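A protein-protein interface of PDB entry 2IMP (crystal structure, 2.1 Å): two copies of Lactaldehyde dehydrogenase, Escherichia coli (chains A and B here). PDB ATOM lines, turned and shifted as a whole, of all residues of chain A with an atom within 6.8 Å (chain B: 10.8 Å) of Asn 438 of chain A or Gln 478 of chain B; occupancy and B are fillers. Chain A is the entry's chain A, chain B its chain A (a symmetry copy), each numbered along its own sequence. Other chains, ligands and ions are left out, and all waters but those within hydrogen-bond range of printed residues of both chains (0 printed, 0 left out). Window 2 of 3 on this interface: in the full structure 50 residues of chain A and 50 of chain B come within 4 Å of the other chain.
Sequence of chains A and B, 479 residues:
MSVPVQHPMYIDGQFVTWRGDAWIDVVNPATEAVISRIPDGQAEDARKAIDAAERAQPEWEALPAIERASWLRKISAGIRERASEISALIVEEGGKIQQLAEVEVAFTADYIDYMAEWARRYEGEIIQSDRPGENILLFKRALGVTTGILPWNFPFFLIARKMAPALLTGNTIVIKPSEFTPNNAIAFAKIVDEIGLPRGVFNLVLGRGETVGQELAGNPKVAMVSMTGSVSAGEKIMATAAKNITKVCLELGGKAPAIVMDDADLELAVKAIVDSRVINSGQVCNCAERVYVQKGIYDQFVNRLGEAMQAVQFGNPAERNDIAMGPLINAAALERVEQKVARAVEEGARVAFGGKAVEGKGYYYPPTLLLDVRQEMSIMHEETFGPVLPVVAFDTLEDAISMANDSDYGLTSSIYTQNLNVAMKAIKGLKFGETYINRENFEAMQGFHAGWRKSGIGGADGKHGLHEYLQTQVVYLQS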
ATOM      1  N   ALA A 264       8.371  28.772   8.013  1.00  0.00           N
ATOM      2  CA  ALA A 264       8.024  27.377   7.811  1.00  0.00           C
ATOM      3  C   ALA A 264       6.533  27.043   7.930  1.00  0.00           C
ATOM      4  O   ALA A 264       5.823  27.602   8.765  1.00  0.00           O
ATOM      5  CB  ALA A 264       8.806  26.510   8.784  1.00  0.00           C
ATOM      6  N   ASP A 265       6.075  26.132   7.077  1.00  0.00           N
ATOM      7  CA  ASP A 265       4.696  25.690   7.126  1.00  0.00           C
ATOM      8  C   ASP A 265       4.405  25.035   8.492  1.00  0.00           C
ATOM      9  O   ASP A 265       4.596  23.831   8.661  1.00  0.00           O
ATOM     10  CB  ASP A 265       4.439  24.680   6.002  1.00  0.00           C
ATOM     11  CG  ASP A 265       2.981  24.272   5.898  1.00  0.00           C
ATOM     12  OD1 ASP A 265       2.414  23.783   6.898  1.00  0.00           O
ATOM     13  OD2 ASP A 265       2.401  24.434   4.802  1.00  0.00           O
ATOM     14  N   LEU A 268       2.595  21.624   8.547  1.00  0.00           N
ATOM     15  CA  LEU A 268       3.442  20.560   8.032  1.00  0.00           C
ATOM     16  C   LEU A 268       4.528  20.133   9.050  1.00  0.00           C
ATOM     17  O   LEU A 268       4.678  18.951   9.360  1.00  0.00           O
ATOM     18  CB  LEU A 268       4.090  21.030   6.723  1.00  0.00           C
ATOM     19  CG  LEU A 268       4.922  20.075   5.859  1.00  0.00           C
ATOM     20  CD1 LEU A 268       5.191  20.733   4.512  1.00  0.00           C
ATOM     21  CD2 LEU A 268       6.231  19.725   6.547  1.00  0.00           C
ATOM     22  N   ALA A 269       5.257  21.116   9.568  1.00  0.00           N
ATOM     23  CA  ALA A 269       6.307  20.858  10.543  1.00  0.00           C
ATOM     24  C   ALA A 269       5.831  20.056  11.769  1.00  0.00           C
ATOM     25  O   ALA A 269       6.427  19.041  12.120  1.00  0.00           O
ATOM     26  CB  ALA A 269       6.929  22.177  10.994  1.00  0.00           C
ATOM     27  N   ALA A 272       4.869  16.489  10.750  1.00  0.00           N
ATOM     28  CA  ALA A 272       6.070  15.739  10.417  1.00  0.00           C
ATOM     29  C   ALA A 272       6.857  15.282  11.661  1.00  0.00           C
ATOM     30  O   ALA A 272       7.390  14.177  11.699  1.00  0.00           O
ATOM     31  CB  ALA A 272       6.971  16.575   9.513  1.00  0.00           C
ATOM     32  N   SER A 414      16.867  17.348   9.734  1.00  0.00           N
ATOM     33  CA  SER A 414      15.731  17.909   9.015  1.00  0.00           C
ATOM     34  C   SER A 414      15.507  19.417   9.229  1.00  0.00           C
ATOM     35  O   SER A 414      15.850  19.970  10.276  1.00  0.00           O
ATOM     36  CB  SER A 414      14.447  17.162   9.386  1.00  0.00           C
ATOM     37  OG  SER A 414      14.055  17.437  10.718  1.00  0.00           O
ATOM     38  N   ILE A 415      14.931  20.063   8.224  1.00  0.00           N
ATOM     39  CA  ILE A 415      14.638  21.483   8.306  1.00  0.00           C
ATOM     40  C   ILE A 415      13.350  21.878   7.561  1.00  0.00           C
ATOM     41  O   ILE A 415      13.005  21.282   6.537  1.00  0.00           O
ATOM     42  CB  ILE A 415      15.814  22.333   7.767  1.00  0.00           C
ATOM     43  CG1 ILE A 415      15.530  23.820   8.004  1.00  0.00           C
ATOM     44  CG2 ILE A 415      16.036  22.049   6.294  1.00  0.00           C
ATOM     45  CD1 ILE A 415      16.680  24.741   7.655  1.00  0.00           C
ATOM     46  N   TYR A 416      12.647  22.869   8.104  1.00  0.00           N
ATOM     47  CA  TYR A 416      11.405  23.358   7.515  1.00  0.00           C
ATOM     48  C   TYR A 416      11.449  24.853   7.193  1.00  0.00           C
ATOM     49  O   TYR A 416      11.554  25.693   8.082  1.00  0.00           O
ATOM     50  CB  TYR A 416      10.238  23.059   8.448  1.00  0.00           C
ATOM     51  CG  TYR A 416      10.169  21.604   8.826  1.00  0.00           C
ATOM     52  CD1 TYR A 416      11.025  21.078   9.792  1.00  0.00           C
ATOM     53  CD2 TYR A 416       9.301  20.733   8.168  1.00  0.00           C
ATOM     54  CE1 TYR A 416      11.025  19.718  10.092  1.00  0.00           C
ATOM     55  CE2 TYR A 416       9.294  19.370   8.460  1.00  0.00           C
ATOM     56  CZ  TYR A 416      10.160  18.872   9.422  1.00  0.00           C
ATOM     57  OH  TYR A 416      10.180  17.524   9.704  1.00  0.00           O
ATOM     58  N   THR A 417      11.374  25.161   5.907  1.00  0.00           N
ATOM     59  CA  THR A 417      11.439  26.531   5.439  1.00  0.00           C
ATOM     60  C   THR A 417      10.941  26.661   3.991  1.00  0.00           C
ATOM     61  O   THR A 417      10.733  25.653   3.311  1.00  0.00           O
ATOM     62  CB  THR A 417      12.898  27.045   5.516  1.00  0.00           C
ATOM     63  OG1 THR A 417      12.978  28.388   5.029  1.00  0.00           O
ATOM     64  CG2 THR A 417      13.809  26.161   4.677  1.00  0.00           C
ATOM     65  N   GLN A 418      10.760  27.893   3.531  1.00  0.00           N
ATOM     66  CA  GLN A 418      10.287  28.115   2.175  1.00  0.00           C
ATOM     67  C   GLN A 418      11.235  28.995   1.327  1.00  0.00           C
ATOM     68  O   GLN A 418      10.934  29.336   0.174  1.00  0.00           O
ATOM     69  CB  GLN A 418       8.884  28.724   2.223  1.00  0.00           C
ATOM     70  CG  GLN A 418       7.955  27.968   3.176  1.00  0.00           C
ATOM     71  CD  GLN A 418       6.536  28.511   3.160  1.00  0.00           C
ATOM     72  OE1 GLN A 418       5.576  27.746   2.962  1.00  0.00           O
ATOM     73  NE2 GLN A 418       6.379  29.803   3.393  1.00  0.00           N
ATOM     74  N   TYR A 436      16.374  15.791   5.705  1.00  0.00           N
ATOM     75  CA  TYR A 436      15.011  15.861   5.199  1.00  0.00           C
ATOM     76  C   TYR A 436      14.456  17.288   5.163  1.00  0.00           C
ATOM     77  O   TYR A 436      14.485  18.001   6.164  1.00  0.00           O
ATOM     78  CB  TYR A 436      14.080  14.987   6.037  1.00  0.00           C
ATOM     79  CG  TYR A 436      14.401  13.521   5.963  1.00  0.00           C
ATOM     80  CD1 TYR A 436      15.363  12.957   6.796  1.00  0.00           C
ATOM     81  CD2 TYR A 436      13.763  12.697   5.038  1.00  0.00           C
ATOM     82  CE1 TYR A 436      15.681  11.604   6.715  1.00  0.00           C
ATOM     83  CE2 TYR A 436      14.072  11.344   4.945  1.00  0.00           C
ATOM     84  CZ  TYR A 436      15.033  10.806   5.786  1.00  0.00           C
ATOM     85  OH  TYR A 436      15.347   9.469   5.698  1.00  0.00           O
ATOM     86  N   ILE A 437      13.967  17.689   3.998  1.00  0.00           N
ATOM     87  CA  ILE A 437      13.409  19.017   3.831  1.00  0.00           C
ATOM     88  C   ILE A 437      11.871  19.034   3.639  1.00  0.00           C
ATOM     89  O   ILE A 437      11.345  18.460   2.680  1.00  0.00           O
ATOM     90  CB  ILE A 437      14.079  19.734   2.648  1.00  0.00           C
ATOM     91  CG1 ILE A 437      15.594  19.784   2.880  1.00  0.00           C
ATOM     92  CG2 ILE A 437      13.517  21.148   2.501  1.00  0.00           C
ATOM     93  CD1 ILE A 437      16.362  20.458   1.768  1.00  0.00           C
ATOM     94  N   ASN A 438      11.186  19.692   4.570  1.00  0.00           N
ATOM     95  CA  ASN A 438       9.732  19.812   4.549  1.00  0.00           C
ATOM     96  C   ASN A 438       8.947  18.487   4.400  1.00  0.00           C
ATOM     97  O   ASN A 438       8.028  18.378   3.591  1.00  0.00           O
ATOM     98  CB  ASN A 438       9.300  20.797   3.459  1.00  0.00           C
ATOM     99  CG  ASN A 438       9.755  22.218   3.748  1.00  0.00           C
ATOM    100  OD1 ASN A 438       9.775  22.652   4.900  1.00  0.00           O
ATOM    101  ND2 ASN A 438      10.112  22.950   2.701  1.00  0.00           N
ATOM    102  N   ARG A 439       9.340  17.504   5.200  1.00  0.00           N
ATOM    103  CA  ARG A 439       8.711  16.188   5.250  1.00  0.00           C
ATOM    104  C   ARG A 439       9.217  15.374   6.452  1.00  0.00           C
ATOM    105  O   ARG A 439      10.184  15.772   7.099  1.00  0.00           O
ATOM    106  CB  ARG A 439       8.963  15.398   3.959  1.00  0.00           C
ATOM    107  CG  ARG A 439      10.429  15.174   3.626  1.00  0.00           C
ATOM    108  CD  ARG A 439      10.638  13.869   2.844  1.00  0.00           C
ATOM    109  NE  ARG A 439      10.505  12.694   3.706  1.00  0.00           N
ATOM    110  CZ  ARG A 439      10.727  11.438   3.321  1.00  0.00           C
ATOM    111  NH1 ARG A 439      11.098  11.168   2.072  1.00  0.00           N
ATOM    112  NH2 ARG A 439      10.585  10.445   4.194  1.00  0.00           N
ATOM    113  N   GLU A 440       8.572  14.251   6.746  1.00  0.00           N
ATOM    114  CA  GLU A 440       8.994  13.439   7.877  1.00  0.00           C
ATOM    115  C   GLU A 440      10.221  12.537   7.594  1.00  0.00           C
ATOM    116  O   GLU A 440      10.533  12.246   6.439  1.00  0.00           O
ATOM    117  CB  GLU A 440       7.816  12.596   8.389  1.00  0.00           C
ATOM    118  CG  GLU A 440       7.463  11.359   7.576  1.00  0.00           C
ATOM    119  CD  GLU A 440       7.017  11.669   6.162  1.00  0.00           C
ATOM    120  OE1 GLU A 440       6.454  12.760   5.921  1.00  0.00           O
ATOM    121  OE2 GLU A 440       7.215  10.803   5.291  1.00  0.00           O
ATOM    122  N   ILE B 127      18.893  10.491  -7.387  1.00  0.00           N
ATOM    123  CA  ILE B 127      18.112   9.267  -7.357  1.00  0.00           C
ATOM    124  C   ILE B 127      16.596   9.429  -7.459  1.00  0.00           C
ATOM    125  O   ILE B 127      16.003  10.260  -6.770  1.00  0.00           O
ATOM    126  CB  ILE B 127      18.426   8.493  -6.055  1.00  0.00           C
ATOM    127  CG1 ILE B 127      19.939   8.284  -5.937  1.00  0.00           C
ATOM    128  CG2 ILE B 127      17.696   7.160  -6.034  1.00  0.00           C
ATOM    129  CD1 ILE B 127      20.395   7.907  -4.529  1.00  0.00           C
ATOM    130  N   SER B 129      12.827   9.072  -6.807  1.00  0.00           N
ATOM    131  CA  SER B 129      12.063   8.810  -5.599  1.00  0.00           C
ATOM    132  C   SER B 129      10.692   8.176  -5.877  1.00  0.00           C
ATOM    133  O   SER B 129      10.168   8.318  -6.976  1.00  0.00           O
ATOM    134  CB  SER B 129      11.853  10.115  -4.837  1.00  0.00           C
ATOM    135  OG  SER B 129      10.897   9.950  -3.809  1.00  0.00           O
ATOM    136  N   ASP B 130      10.141   7.463  -4.898  1.00  0.00           N
ATOM    137  CA  ASP B 130       8.806   6.882  -5.052  1.00  0.00           C
ATOM    138  C   ASP B 130       7.711   7.947  -4.774  1.00  0.00           C
ATOM    139  O   ASP B 130       6.538   7.760  -5.107  1.00  0.00           O
ATOM    140  CB  ASP B 130       8.592   5.714  -4.079  1.00  0.00           C
ATOM    141  CG  ASP B 130       9.405   4.488  -4.432  1.00  0.00           C
ATOM    142  OD1 ASP B 130      10.182   4.530  -5.405  1.00  0.00           O
ATOM    143  OD2 ASP B 130       9.266   3.470  -3.728  1.00  0.00           O
ATOM    144  N   ARG B 131       8.135   9.051  -4.156  1.00  0.00           N
ATOM    145  CA  ARG B 131       7.239  10.145  -3.799  1.00  0.00           C
ATOM    146  C   ARG B 131       7.092  11.248  -4.850  1.00  0.00           C
ATOM    147  O   ARG B 131       8.085  11.818  -5.307  1.00  0.00           O
ATOM    148  CB  ARG B 131       7.699  10.811  -2.504  1.00  0.00           C
ATOM    149  CG  ARG B 131       7.797   9.888  -1.318  1.00  0.00           C
ATOM    150  CD  ARG B 131       7.945  10.700  -0.048  1.00  0.00           C
ATOM    151  NE  ARG B 131       8.001   9.839   1.124  1.00  0.00           N
ATOM    152  CZ  ARG B 131       7.763  10.252   2.364  1.00  0.00           C
ATOM    153  NH1 ARG B 131       7.447  11.519   2.593  1.00  0.00           N
ATOM    154  NH2 ARG B 131       7.844   9.394   3.370  1.00  0.00           N
ATOM    155  N   PRO B 132       5.843  11.569  -5.224  1.00  0.00           N
ATOM    156  CA  PRO B 132       5.557  12.605  -6.215  1.00  0.00           C
ATOM    157  C   PRO B 132       6.215  13.949  -5.822  1.00  0.00           C
ATOM    158  O   PRO B 132       6.115  14.390  -4.674  1.00  0.00           O
ATOM    159  CB  PRO B 132       4.031  12.693  -6.187  1.00  0.00           C
ATOM    160  CG  PRO B 132       3.621  11.309  -5.854  1.00  0.00           C
ATOM    161  CD  PRO B 132       4.596  10.930  -4.764  1.00  0.00           C
ATOM    162  N   GLY B 133       6.889  14.574  -6.781  1.00  0.00           N
ATOM    163  CA  GLY B 133       7.515  15.859  -6.523  1.00  0.00           C
ATOM    164  C   GLY B 133       8.735  15.865  -5.619  1.00  0.00           C
ATOM    165  O   GLY B 133       9.220  16.935  -5.248  1.00  0.00           O
ATOM    166  N   GLU B 134       9.230  14.689  -5.240  1.00  0.00           N
ATOM    167  CA  GLU B 134      10.414  14.645  -4.394  1.00  0.00           C
ATOM    168  C   GLU B 134      11.713  14.346  -5.153  1.00  0.00           C
ATOM    169  O   GLU B 134      11.742  13.523  -6.065  1.00  0.00           O
ATOM    170  CB  GLU B 134      10.266  13.608  -3.270  1.00  0.00           C
ATOM    171  CG  GLU B 134      11.544  13.450  -2.430  1.00  0.00           C
ATOM    172  CD  GLU B 134      11.429  12.423  -1.308  1.00  0.00           C
ATOM    173  OE1 GLU B 134      11.460  11.210  -1.590  1.00  0.00           O
ATOM    174  OE2 GLU B 134      11.313  12.832  -0.136  1.00  0.00           O
ATOM    175  N   ASN B 135      12.771  15.043  -4.768  1.00  0.00           N
ATOM    176  CA  ASN B 135      14.092  14.833  -5.338  1.00  0.00           C
ATOM    177  C   ASN B 135      15.066  14.272  -4.293  1.00  0.00           C
ATOM    178  O   ASN B 135      15.203  14.836  -3.205  1.00  0.00           O
ATOM    179  CB  ASN B 135      14.689  16.140  -5.868  1.00  0.00           C
ATOM    180  CG  ASN B 135      14.158  16.523  -7.233  1.00  0.00           C
ATOM    181  OD1 ASN B 135      14.254  15.751  -8.189  1.00  0.00           O
ATOM    182  ND2 ASN B 135      13.607  17.727  -7.334  1.00  0.00           N
ATOM    183  N   ILE B 136      15.711  13.160  -4.613  1.00  0.00           N
ATOM    184  CA  ILE B 136      16.683  12.584  -3.709  1.00  0.00           C
ATOM    185  C   ILE B 136      18.103  12.910  -4.190  1.00  0.00           C
ATOM    186  O   ILE B 136      18.584  12.343  -5.170  1.00  0.00           O
ATOM    187  CB  ILE B 136      16.523  11.057  -3.605  1.00  0.00           C
ATOM    188  CG1 ILE B 136      15.123  10.711  -3.093  1.00  0.00           C
ATOM    189  CG2 ILE B 136      17.569  10.494  -2.663  1.00  0.00           C
ATOM    190  CD1 ILE B 136      14.819   9.224  -3.102  1.00  0.00           C
ATOM    191  N   LEU B 137      18.733  13.859  -3.512  1.00  0.00           N
ATOM    192  CA  LEU B 137      20.068  14.296  -3.866  1.00  0.00           C
ATOM    193  C   LEU B 137      21.168  13.719  -2.976  1.00  0.00           C
ATOM    194  O   LEU B 137      21.183  13.951  -1.770  1.00  0.00           O
ATOM    195  CB  LEU B 137      20.147  15.828  -3.812  1.00  0.00           C
ATOM    196  CG  LEU B 137      19.067  16.591  -4.581  1.00  0.00           C
ATOM    197  CD1 LEU B 137      19.236  18.083  -4.343  1.00  0.00           C
ATOM    198  CD2 LEU B 137      19.155  16.260  -6.061  1.00  0.00           C
ATOM    199  N   VAL B 474      22.703  12.341   1.973  1.00  0.00           N
ATOM    200  CA  VAL B 474      21.489  12.157   1.204  1.00  0.00           C
ATOM    201  C   VAL B 474      20.387  13.146   1.582  1.00  0.00           C
ATOM    202  O   VAL B 474      19.891  13.155   2.717  1.00  0.00           O
ATOM    203  CB  VAL B 474      20.956  10.710   1.341  1.00  0.00           C
ATOM    204  CG1 VAL B 474      19.689  10.537   0.519  1.00  0.00           C
ATOM    205  CG2 VAL B 474      22.018   9.725   0.869  1.00  0.00           C
ATOM    206  N   VAL B 475      20.029  13.986   0.620  1.00  0.00           N
ATOM    207  CA  VAL B 475      19.002  14.986   0.834  1.00  0.00           C
ATOM    208  C   VAL B 475      17.640  14.648   0.199  1.00  0.00           C
ATOM    209  O   VAL B 475      17.536  14.450  -1.015  1.00  0.00           O
ATOM    210  CB  VAL B 475      19.451  16.363   0.296  1.00  0.00           C
ATOM    211  CG1 VAL B 475      18.392  17.415   0.603  1.00  0.00           C
ATOM    212  CG2 VAL B 475      20.789  16.752   0.924  1.00  0.00           C
ATOM    213  N   TYR B 476      16.618  14.560   1.041  1.00  0.00           N
ATOM    214  CA  TYR B 476      15.274  14.302   0.562  1.00  0.00           C
ATOM    215  C   TYR B 476      14.495  15.623   0.467  1.00  0.00           C
ATOM    216  O   TYR B 476      13.932  16.108   1.452  1.00  0.00           O
ATOM    217  CB  TYR B 476      14.540  13.324   1.483  1.00  0.00           C
ATOM    218  CG  TYR B 476      15.125  11.926   1.520  1.00  0.00           C
ATOM    219  CD1 TYR B 476      16.241  11.633   2.301  1.00  0.00           C
ATOM    220  CD2 TYR B 476      14.546  10.885   0.788  1.00  0.00           C
ATOM    221  CE1 TYR B 476      16.762  10.337   2.364  1.00  0.00           C
ATOM    222  CE2 TYR B 476      15.063   9.586   0.842  1.00  0.00           C
ATOM    223  CZ  TYR B 476      16.173   9.323   1.633  1.00  0.00           C
ATOM    224  OH  TYR B 476      16.691   8.045   1.696  1.00  0.00           O
ATOM    225  N   LEU B 477      14.525  16.209  -0.720  1.00  0.00           N
ATOM    226  CA  LEU B 477      13.859  17.474  -0.967  1.00  0.00           C
ATOM    227  C   LEU B 477      12.397  17.302  -1.428  1.00  0.00           C
ATOM    228  O   LEU B 477      12.134  17.021  -2.597  1.00  0.00           O
ATOM    229  CB  LEU B 477      14.666  18.259  -2.004  1.00  0.00           C
ATOM    230  CG  LEU B 477      14.272  19.702  -2.311  1.00  0.00           C
ATOM    231  CD1 LEU B 477      14.043  20.473  -1.021  1.00  0.00           C
ATOM    232  CD2 LEU B 477      15.380  20.348  -3.129  1.00  0.00           C
ATOM    233  N   GLN B 478      11.466  17.457  -0.489  1.00  0.00           N
ATOM    234  CA  GLN B 478      10.045  17.300  -0.787  1.00  0.00           C
ATOM    235  C   GLN B 478       9.357  18.549  -1.380  1.00  0.00           C
ATOM    236  O   GLN B 478       9.360  19.621  -0.773  1.00  0.00           O
ATOM    237  CB  GLN B 478       9.288  16.862   0.469  1.00  0.00           C
ATOM    238  CG  GLN B 478       7.806  16.602   0.230  1.00  0.00           C
ATOM    239  CD  GLN B 478       7.566  15.448  -0.729  1.00  0.00           C
ATOM    240  OE1 GLN B 478       7.779  14.281  -0.383  1.00  0.00           O
ATOM    241  NE2 GLN B 478       7.133  15.769  -1.946  1.00  0.00           N
ATOM    242  N   SER B 479       8.771  18.371  -2.562  1.00  0.00           N
ATOM    243  CA  SER B 479       8.076  19.442  -3.269  1.00  0.00           C
ATOM    244  C   SER B 479       8.996  20.564  -3.790  1.00  0.00           C
ATOM    245  O   SER B 479       9.430  20.536  -4.941  1.00  0.00           O
ATOM    246  CB  SER B 479       6.991  20.048  -2.376  1.00  0.00           C
ATOM    247  OG  SER B 479       6.350  21.137  -3.019  1.00  0.00           O
ATOM    248  OXT SER B 479       9.104  21.403  -2.935  1.00  0.00           O
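O of Asn 135 of chain B sits at hydrogen-bond distance from N of Leu 477 of chain B, 2.9 Å away.
OG of Ser 129 of chain B sits at hydrogen-bond distance from N of Arg 131 of chain B, at 2.9 Å.
N of Ile 415 of chain A sits at hydrogen-bond distance from O of Tyr 436 of chain A.
The backbone NH of Asn 438 of chain A lies within hydrogen-bond range of the backbone carbonyl oxygen of Ile 415 of chain A (3.1 Å).
The backbone carbonyl oxygen (O) of Arg 439 of chain A is in hydrogen-bond range of the side-chain hydroxyl (OH) of Tyr 416 of chain A (3.1 Å).
N of Val 475 of chain B is in hydrogen-bond range of O of Leu 137 of chain B (2.7 Å).
CE2 of Tyr 436 of chain A touches CD1 of Tyr 476 of chain B, 3.4 Å away.
CG1 of Val 475 of chain B touches CD1 of Ile 437 of chain A, 3.8 Å away.
CD1 of Leu 477 of chain B touches CG2 of Ile 437 of chain A, at 3.6 Å.
Asn 438 of chain A touches Gln 478 of chain B (O to CB, 3.7 Å).
Arg 439 of chain A touches Tyr 476 of chain B (NH1 to CD2, 3.7 Å).
Gln 478 of chain B touches Arg 439 of chain A.
O of Ile 437 of chain A sits at hydrogen-bond distance from N of Gln 478 of chain B (3.3 Å).
NH2 of Arg 131 of chain B lies close to NH2 of Arg 439 of chain A, 3.0 Å away.
NH1 of Arg 439 of chain A is in salt-bridge range of OE2 of Glu 134 of chain B (2.8 Å).
The side-chain carboxylate of Glu 440 of chain A is in salt-bridge range of the guanidinium group of Arg 131 of chain B (2.5 Å).
The backbone NH (N) of Ile 437 of chain A sits at hydrogen-bond distance from the backbone carbonyl oxygen (O) of Tyr 476 of chain B (3.0 Å).
Along chain A the printed residues that touch a printed residue of chain B span positions 436 to 440.
Hydrophobic or aromatic side chains of chain B that line the printed part of chain A: Val 475, Tyr 476 and Leu 477.
Among the printed residues, 11 pairs touch across the chains.
Among the printed residues, Asp or Glu carboxylates within 4 Å of a Lys or Arg side-chain nitrogen of the other chain: Arg 439 of chain A with Glu 134 of chain B (2.8 Å) and Glu 440 of chain A with Arg 131 of chain B (2.5 Å).
No position is printed for both chains.
No residue of chain B comes within 4 Å of Tyr 416 of chain A.
No residue of chain B comes within 4 Å of Thr 417 of chain A.
Gln 418 of chain A touches none of the printed residues of chain B.
Of chain B, only Arg 131, Glu 134, Tyr 476 and Gln 478 come within 4 Å of Arg 439 of chain A.
Of the printed residues of chain B, Glu 440 of chain A touches Arg 131 (2.5 Å).
Of the printed residues of chain A, Glu 134 of chain B touches Arg 439 (2.8 Å).
Asn 135 of chain B touches none of the printed residues of chain A.
Of the printed residues of chain A, Val 475 of chain B touches Ile 437 (3.8 Å).
Of the printed residues of chain A, Leu 477 of chain B touches Ile 437.
The nearest residue of chain B that does not touch Asn 438 of chain A is Tyr 476 of chain B (5.5 Å).
The nearest printed residue of chain A that does not touch Arg 131 of chain B is Tyr 436 of chain A (6.7 Å).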
